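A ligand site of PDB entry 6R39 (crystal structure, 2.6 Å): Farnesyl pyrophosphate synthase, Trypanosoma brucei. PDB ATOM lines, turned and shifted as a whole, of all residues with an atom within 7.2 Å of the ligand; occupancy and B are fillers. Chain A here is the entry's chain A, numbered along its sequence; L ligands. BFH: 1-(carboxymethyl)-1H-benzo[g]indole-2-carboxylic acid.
N of Asn 51 lies within hydrogen-bond range of O1 of the ligand (3.3 Å). NH2 of Arg 52 lies within salt-bridge range of O3 of the ligand (2.8 Å).
N of Arg 52 lies within hydrogen-bond range of OE1 of Glu 95 (3.4 Å). The side-chain hydroxyl of Thr 364 lies within hydrogen-bond range of the backbone carbonyl oxygen of Leu 360 (3.0 Å). OH of Tyr 220 lies within hydrogen-bond range of OG1 of Thr 364, at 3.1 Å. OG1 of Thr 55 sits at hydrogen-bond distance from O of Asn 51. The side-chain hydroxyl (OG1) of Thr 219 is in hydrogen-bond range of the guanidinium group (NH1) of Arg 52, at 3.0 Å. The guanidinium group of Arg 52 is in hydrogen-bond range of the side-chain hydroxyl of Tyr 218, 3.5 Å away.
Residues that only touch the ligand: Lys 49 (3.3 Å), Tyr 50 (3.7 Å), Thr 219 (3.3 Å), Tyr 220 (3.5 Å), Leu 360 (3.5 Å), Lys 363 (3.7 Å) and Thr 364 (3.7 Å). Hydrophobic or aromatic side chains within 4 Å of the ligand: Tyr 220 and Leu 360.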
ATOM      1  N   GLY A  48      -1.848 -16.868   5.644  1.00  0.00           N
ATOM      2  CA  GLY A  48      -1.065 -16.268   4.572  1.00  0.00           C
ATOM      3  C   GLY A  48       0.055 -17.131   4.015  1.00  0.00           C
ATOM      4  O   GLY A  48       0.098 -18.345   4.269  1.00  0.00           O
ATOM      5  N   LYS A  49       0.944 -16.513   3.229  1.00  0.00           N
ATOM      6  CA  LYS A  49       2.058 -17.262   2.647  1.00  0.00           C
ATOM      7  C   LYS A  49       3.313 -17.125   3.506  1.00  0.00           C
ATOM      8  O   LYS A  49       4.281 -17.848   3.282  1.00  0.00           O
ATOM      9  CB  LYS A  49       2.297 -16.884   1.169  1.00  0.00           C
ATOM     10  CG  LYS A  49       2.885 -17.998   0.315  1.00  0.00           C
ATOM     11  CD  LYS A  49       3.132 -17.509  -1.111  1.00  0.00           C
ATOM     12  CE  LYS A  49       4.070 -18.384  -1.895  1.00  0.00           C
ATOM     13  NZ  LYS A  49       4.425 -17.765  -3.192  1.00  0.00           N
ATOM     14  N   TYR A  50       3.261 -16.213   4.528  1.00  0.00           N
ATOM     15  CA  TYR A  50       4.332 -15.941   5.496  1.00  0.00           C
ATOM     16  C   TYR A  50       5.583 -15.387   4.846  1.00  0.00           C
ATOM     17  O   TYR A  50       6.672 -15.547   5.398  1.00  0.00           O
ATOM     18  CB  TYR A  50       4.677 -17.211   6.328  1.00  0.00           C
ATOM     19  CG  TYR A  50       3.460 -17.929   6.864  1.00  0.00           C
ATOM     20  CD1 TYR A  50       2.717 -17.392   7.904  1.00  0.00           C
ATOM     21  CD2 TYR A  50       3.029 -19.131   6.309  1.00  0.00           C
ATOM     22  CE1 TYR A  50       1.570 -18.026   8.382  1.00  0.00           C
ATOM     23  CE2 TYR A  50       1.900 -19.788   6.793  1.00  0.00           C
ATOM     24  CZ  TYR A  50       1.162 -19.233   7.822  1.00  0.00           C
ATOM     25  OH  TYR A  50       0.043 -19.877   8.281  1.00  0.00           O
ATOM     26  N   ASN A  51       5.425 -14.719   3.694  1.00  0.00           N
ATOM     27  CA  ASN A  51       6.576 -14.225   2.934  1.00  0.00           C
ATOM     28  C   ASN A  51       7.411 -13.185   3.698  1.00  0.00           C
ATOM     29  O   ASN A  51       8.622 -13.257   3.546  1.00  0.00           O
ATOM     30  CB  ASN A  51       6.208 -13.792   1.541  1.00  0.00           C
ATOM     31  CG  ASN A  51       6.183 -14.953   0.544  1.00  0.00           C
ATOM     32  OD1 ASN A  51       6.986 -15.901   0.611  1.00  0.00           O
ATOM     33  ND2 ASN A  51       5.263 -14.917  -0.410  1.00  0.00           N
ATOM     34  N   ARG A  52       6.821 -12.346   4.605  1.00  0.00           N
ATOM     35  CA  ARG A  52       7.614 -11.414   5.437  1.00  0.00           C
ATOM     36  C   ARG A  52       8.455 -12.187   6.470  1.00  0.00           C
ATOM     37  O   ARG A  52       9.649 -11.923   6.632  1.00  0.00           O
ATOM     38  CB  ARG A  52       6.712 -10.394   6.146  1.00  0.00           C
ATOM     39  CG  ARG A  52       6.400  -9.153   5.336  1.00  0.00           C
ATOM     40  CD  ARG A  52       5.275  -8.392   6.004  1.00  0.00           C
ATOM     41  NE  ARG A  52       4.543  -7.497   5.096  1.00  0.00           N
ATOM     42  CZ  ARG A  52       3.638  -7.899   4.209  1.00  0.00           C
ATOM     43  NH1 ARG A  52       3.024  -7.013   3.441  1.00  0.00           N
ATOM     44  NH2 ARG A  52       3.392  -9.195   4.030  1.00  0.00           N
ATOM     45  N   GLY A  53       7.814 -13.134   7.150  1.00  0.00           N
ATOM     46  CA  GLY A  53       8.469 -13.975   8.154  1.00  0.00           C
ATOM     47  C   GLY A  53       9.530 -14.893   7.603  1.00  0.00           C
ATOM     48  O   GLY A  53      10.649 -14.965   8.144  1.00  0.00           O
ATOM     49  N   THR A  55      11.239 -14.471   4.891  1.00  0.00           N
ATOM     50  CA  THR A  55      12.351 -13.613   4.451  1.00  0.00           C
ATOM     51  C   THR A  55      13.417 -13.489   5.554  1.00  0.00           C
ATOM     52  O   THR A  55      14.595 -13.465   5.247  1.00  0.00           O
ATOM     53  CB  THR A  55      11.838 -12.250   3.906  1.00  0.00           C
ATOM     54  OG1 THR A  55      11.000 -12.500   2.779  1.00  0.00           O
ATOM     55  CG2 THR A  55      12.968 -11.300   3.489  1.00  0.00           C
ATOM     56  N   GLU A  95       5.057 -11.007  11.279  1.00  0.00           N
ATOM     57  CA  GLU A  95       3.775 -11.643  10.958  1.00  0.00           C
ATOM     58  C   GLU A  95       2.652 -11.195  11.915  1.00  0.00           C
ATOM     59  O   GLU A  95       1.559 -10.898  11.450  1.00  0.00           O
ATOM     60  CB  GLU A  95       3.872 -13.180  10.883  1.00  0.00           C
ATOM     61  CG  GLU A  95       4.692 -13.703   9.700  1.00  0.00           C
ATOM     62  CD  GLU A  95       4.172 -13.398   8.294  1.00  0.00           C
ATOM     63  OE1 GLU A  95       5.009 -13.137   7.397  1.00  0.00           O
ATOM     64  OE2 GLU A  95       2.939 -13.413   8.097  1.00  0.00           O
ATOM     65  N   GLN A  98       1.905  -7.539  11.092  1.00  0.00           N
ATOM     66  CA  GLN A  98       1.117  -7.573   9.863  1.00  0.00           C
ATOM     67  C   GLN A  98      -0.311  -7.968  10.212  1.00  0.00           C
ATOM     68  O   GLN A  98      -1.242  -7.298   9.766  1.00  0.00           O
ATOM     69  CB  GLN A  98       1.756  -8.504   8.815  1.00  0.00           C
ATOM     70  CG  GLN A  98       0.877  -8.934   7.631  1.00  0.00           C
ATOM     71  CD  GLN A  98       0.536  -7.839   6.655  1.00  0.00           C
ATOM     72  OE1 GLN A  98       0.758  -6.659   6.881  1.00  0.00           O
ATOM     73  NE2 GLN A  98      -0.033  -8.234   5.532  1.00  0.00           N
ATOM     74  N   TYR A 218       8.000  -1.781   6.403  1.00  0.00           N
ATOM     75  CA  TYR A 218       7.711  -2.993   7.190  1.00  0.00           C
ATOM     76  C   TYR A 218       7.713  -4.297   6.330  1.00  0.00           C
ATOM     77  O   TYR A 218       7.987  -5.364   6.870  1.00  0.00           O
ATOM     78  CB  TYR A 218       6.402  -2.830   8.034  1.00  0.00           C
ATOM     79  CG  TYR A 218       5.121  -3.303   7.366  1.00  0.00           C
ATOM     80  CD1 TYR A 218       4.465  -2.492   6.443  1.00  0.00           C
ATOM     81  CD2 TYR A 218       4.566  -4.534   7.669  1.00  0.00           C
ATOM     82  CE1 TYR A 218       3.306  -2.926   5.798  1.00  0.00           C
ATOM     83  CE2 TYR A 218       3.400  -4.977   7.040  1.00  0.00           C
ATOM     84  CZ  TYR A 218       2.771  -4.167   6.103  1.00  0.00           C
ATOM     85  OH  TYR A 218       1.632  -4.566   5.438  1.00  0.00           O
ATOM     86  N   THR A 219       7.419  -4.206   5.032  1.00  0.00           N
ATOM     87  CA  THR A 219       7.335  -5.382   4.161  1.00  0.00           C
ATOM     88  C   THR A 219       8.690  -5.797   3.585  1.00  0.00           C
ATOM     89  O   THR A 219       8.958  -7.000   3.474  1.00  0.00           O
ATOM     90  CB  THR A 219       6.312  -5.127   3.056  1.00  0.00           C
ATOM     91  OG1 THR A 219       5.067  -4.793   3.644  1.00  0.00           O
ATOM     92  CG2 THR A 219       6.104  -6.301   2.146  1.00  0.00           C
ATOM     93  N   TYR A 220       9.526  -4.824   3.156  1.00  0.00           N
ATOM     94  CA  TYR A 220      10.810  -5.124   2.555  1.00  0.00           C
ATOM     95  C   TYR A 220      12.004  -4.801   3.432  1.00  0.00           C
ATOM     96  O   TYR A 220      12.866  -5.655   3.552  1.00  0.00           O
ATOM     97  CB  TYR A 220      10.952  -4.480   1.173  1.00  0.00           C
ATOM     98  CG  TYR A 220      10.079  -5.166   0.165  1.00  0.00           C
ATOM     99  CD1 TYR A 220      10.525  -6.283  -0.542  1.00  0.00           C
ATOM    100  CD2 TYR A 220       8.757  -4.770  -0.023  1.00  0.00           C
ATOM    101  CE1 TYR A 220       9.698  -6.970  -1.422  1.00  0.00           C
ATOM    102  CE2 TYR A 220       7.926  -5.430  -0.914  1.00  0.00           C
ATOM    103  CZ  TYR A 220       8.398  -6.539  -1.606  1.00  0.00           C
ATOM    104  OH  TYR A 220       7.574  -7.228  -2.461  1.00  0.00           O
ATOM    105  N   PRO A 223      12.031  -7.102   7.292  1.00  0.00           N
ATOM    106  CA  PRO A 223      12.444  -8.524   7.276  1.00  0.00           C
ATOM    107  C   PRO A 223      13.908  -8.732   6.947  1.00  0.00           C
ATOM    108  O   PRO A 223      14.550  -9.536   7.625  1.00  0.00           O
ATOM    109  CB  PRO A 223      11.510  -9.158   6.237  1.00  0.00           C
ATOM    110  CG  PRO A 223      10.322  -8.261   6.188  1.00  0.00           C
ATOM    111  CD  PRO A 223      10.916  -6.880   6.339  1.00  0.00           C
ATOM    112  N   PHE A 253       6.338  -3.998  -6.057  1.00  0.00           N
ATOM    113  CA  PHE A 253       5.245  -4.771  -5.488  1.00  0.00           C
ATOM    114  C   PHE A 253       3.941  -3.993  -5.444  1.00  0.00           C
ATOM    115  O   PHE A 253       2.916  -4.558  -5.814  1.00  0.00           O
ATOM    116  CB  PHE A 253       5.605  -5.258  -4.080  1.00  0.00           C
ATOM    117  CG  PHE A 253       4.610  -6.193  -3.453  1.00  0.00           C
ATOM    118  CD1 PHE A 253       4.530  -7.526  -3.851  1.00  0.00           C
ATOM    119  CD2 PHE A 253       3.758  -5.754  -2.450  1.00  0.00           C
ATOM    120  CE1 PHE A 253       3.606  -8.387  -3.287  1.00  0.00           C
ATOM    121  CE2 PHE A 253       2.846  -6.624  -1.863  1.00  0.00           C
ATOM    122  CZ  PHE A 253       2.783  -7.949  -2.274  1.00  0.00           C
ATOM    123  N   THR A 359      16.213 -13.880  -4.012  1.00  0.00           N
ATOM    124  CA  THR A 359      15.069 -14.783  -3.805  1.00  0.00           C
ATOM    125  C   THR A 359      13.821 -13.935  -3.479  1.00  0.00           C
ATOM    126  O   THR A 359      12.749 -14.183  -4.045  1.00  0.00           O
ATOM    127  CB  THR A 359      15.441 -15.913  -2.774  1.00  0.00           C
ATOM    128  OG1 THR A 359      16.077 -17.012  -3.442  1.00  0.00           O
ATOM    129  CG2 THR A 359      14.234 -16.450  -2.012  1.00  0.00           C
ATOM    130  N   LEU A 360      13.983 -12.884  -2.632  1.00  0.00           N
ATOM    131  CA  LEU A 360      12.901 -11.958  -2.281  1.00  0.00           C
ATOM    132  C   LEU A 360      12.379 -11.317  -3.548  1.00  0.00           C
ATOM    133  O   LEU A 360      11.182 -11.349  -3.814  1.00  0.00           O
ATOM    134  CB  LEU A 360      13.405 -10.890  -1.260  1.00  0.00           C
ATOM    135  CG  LEU A 360      12.378  -9.893  -0.676  1.00  0.00           C
ATOM    136  CD1 LEU A 360      11.195 -10.593  -0.031  1.00  0.00           C
ATOM    137  CD2 LEU A 360      13.037  -8.956   0.312  1.00  0.00           C
ATOM    138  N   TRP A 361      13.300 -10.860  -4.387  1.00  0.00           N
ATOM    139  CA  TRP A 361      12.990 -10.276  -5.684  1.00  0.00           C
ATOM    140  C   TRP A 361      12.264 -11.238  -6.640  1.00  0.00           C
ATOM    141  O   TRP A 361      11.252 -10.839  -7.221  1.00  0.00           O
ATOM    142  CB  TRP A 361      14.247  -9.681  -6.345  1.00  0.00           C
ATOM    143  CG  TRP A 361      14.004  -9.213  -7.752  1.00  0.00           C
ATOM    144  CD1 TRP A 361      14.600  -9.683  -8.877  1.00  0.00           C
ATOM    145  CD2 TRP A 361      13.041  -8.251  -8.183  1.00  0.00           C
ATOM    146  NE1 TRP A 361      14.124  -9.026  -9.983  1.00  0.00           N
ATOM    147  CE2 TRP A 361      13.140  -8.155  -9.585  1.00  0.00           C
ATOM    148  CE3 TRP A 361      12.122  -7.418  -7.512  1.00  0.00           C
ATOM    149  CZ2 TRP A 361      12.379  -7.255 -10.332  1.00  0.00           C
ATOM    150  CZ3 TRP A 361      11.353  -6.549  -8.243  1.00  0.00           C
ATOM    151  CH2 TRP A 361      11.482  -6.464  -9.638  1.00  0.00           C
ATOM    152  N   GLY A 362      12.747 -12.463  -6.784  1.00  0.00           N
ATOM    153  CA  GLY A 362      12.122 -13.482  -7.620  1.00  0.00           C
ATOM    154  C   GLY A 362      10.653 -13.687  -7.279  1.00  0.00           C
ATOM    155  O   GLY A 362       9.804 -13.715  -8.177  1.00  0.00           O
ATOM    156  N   LYS A 363      10.344 -13.768  -5.943  1.00  0.00           N
ATOM    157  CA  LYS A 363       8.992 -13.903  -5.393  1.00  0.00           C
ATOM    158  C   LYS A 363       8.106 -12.717  -5.801  1.00  0.00           C
ATOM    159  O   LYS A 363       6.961 -12.921  -6.226  1.00  0.00           O
ATOM    160  CB  LYS A 363       9.034 -14.022  -3.861  1.00  0.00           C
ATOM    161  CG  LYS A 363       9.690 -15.296  -3.341  1.00  0.00           C
ATOM    162  CD  LYS A 363       9.499 -15.485  -1.823  1.00  0.00           C
ATOM    163  CE  LYS A 363      10.742 -15.184  -1.024  1.00  0.00           C
ATOM    164  NZ  LYS A 363      10.722 -15.876   0.285  1.00  0.00           N
ATOM    165  N   THR A 364       8.656 -11.474  -5.722  1.00  0.00           N
ATOM    166  CA  THR A 364       7.991 -10.214  -6.082  1.00  0.00           C
ATOM    167  C   THR A 364       7.747 -10.132  -7.596  1.00  0.00           C
ATOM    168  O   THR A 364       6.635  -9.809  -8.006  1.00  0.00           O
ATOM    169  CB  THR A 364       8.809  -9.008  -5.586  1.00  0.00           C
ATOM    170  OG1 THR A 364       9.145  -9.197  -4.216  1.00  0.00           O
ATOM    171  CG2 THR A 364       8.083  -7.683  -5.777  1.00  0.00           C
ATOM    172  N   TYR A 365       8.796 -10.442  -8.397  1.00  0.00           N
ATOM    173  CA  TYR A 365       8.833 -10.431  -9.871  1.00  0.00           C
ATOM    174  C   TYR A 365       7.798 -11.392 -10.466  1.00  0.00           C
ATOM    175  O   TYR A 365       7.216 -11.064 -11.507  1.00  0.00           O
ATOM    176  CB  TYR A 365      10.264 -10.727 -10.349  1.00  0.00           C
ATOM    177  CG  TYR A 365      10.457 -10.678 -11.835  1.00  0.00           C
ATOM    178  CD1 TYR A 365      10.464 -11.846 -12.605  1.00  0.00           C
ATOM    179  CD2 TYR A 365      10.688  -9.467 -12.501  1.00  0.00           C
ATOM    180  CE1 TYR A 365      10.646 -11.808 -13.981  1.00  0.00           C
ATOM    181  CE2 TYR A 365      10.915  -9.422 -13.878  1.00  0.00           C
ATOM    182  CZ  TYR A 365      10.889 -10.599 -14.618  1.00  0.00           C
ATOM    183  OH  TYR A 365      11.089 -10.554 -15.982  1.00  0.00           O
ATOM    184  N   LYS A 366       7.516 -12.534  -9.771  1.00  0.00           N
ATOM    185  CA  LYS A 366       6.506 -13.543 -10.127  1.00  0.00           C
ATOM    186  C   LYS A 366       5.330 -13.447  -9.134  1.00  0.00           C
ATOM    187  O   LYS A 366       4.214 -13.899  -9.417  1.00  0.00           O
ATOM    188  CB  LYS A 366       7.111 -14.957 -10.084  1.00  0.00           C
ATOM    189  CG  LYS A 366       8.056 -15.289 -11.231  1.00  0.00           C
ATOM    190  CD  LYS A 366       8.225 -16.800 -11.408  1.00  0.00           C
ATOM    191  CE  LYS A 366       7.131 -17.442 -12.251  1.00  0.00           C
ATOM    192  NZ  LYS A 366       6.979 -18.891 -11.941  1.00  0.00           N
HETATM  193  O1  BFH L   1       2.901 -13.688   1.884  1.00  0.00           O
HETATM  194  C2  BFH L   1       2.934 -12.476   1.880  1.00  0.00           C
HETATM  195  O3  BFH L   1       3.346 -11.781   2.947  1.00  0.00           O
HETATM  196  C4  BFH L   1       2.485 -11.691   0.662  1.00  0.00           C
HETATM  197  N5  BFH L   1       3.217 -12.052  -0.576  1.00  0.00           N
HETATM  198  C6  BFH L   1       2.665 -12.761  -1.562  1.00  0.00           C
HETATM  199  C7  BFH L   1       3.548 -12.942  -2.554  1.00  0.00           C
HETATM  200  C8  BFH L   1       4.784 -12.195  -2.154  1.00  0.00           C
HETATM  201  C9  BFH L   1       6.023 -12.061  -2.799  1.00  0.00           C
HETATM  202  C10 BFH L   1       7.000 -11.311  -2.139  1.00  0.00           C
HETATM  203  C11 BFH L   1       6.731 -10.742  -0.874  1.00  0.00           C
HETATM  204  C12 BFH L   1       7.757  -9.982  -0.285  1.00  0.00           C
HETATM  205  C13 BFH L   1       7.589  -9.395   0.970  1.00  0.00           C
HETATM  206  C14 BFH L   1       6.366  -9.565   1.626  1.00  0.00           C
HETATM  207  C15 BFH L   1       5.321 -10.247   1.012  1.00  0.00           C
HETATM  208  C16 BFH L   1       5.466 -10.860  -0.243  1.00  0.00           C
HETATM  209  C17 BFH L   1       4.473 -11.628  -0.919  1.00  0.00           C
HETATM  210  C18 BFH L   1       1.359 -13.471  -1.606  1.00  0.00           C
HETATM  211  O19 BFH L   1       1.328 -14.762  -1.985  1.00  0.00           O
HETATM  212  O20 BFH L   1       0.329 -12.900  -1.297  1.00  0.00           O
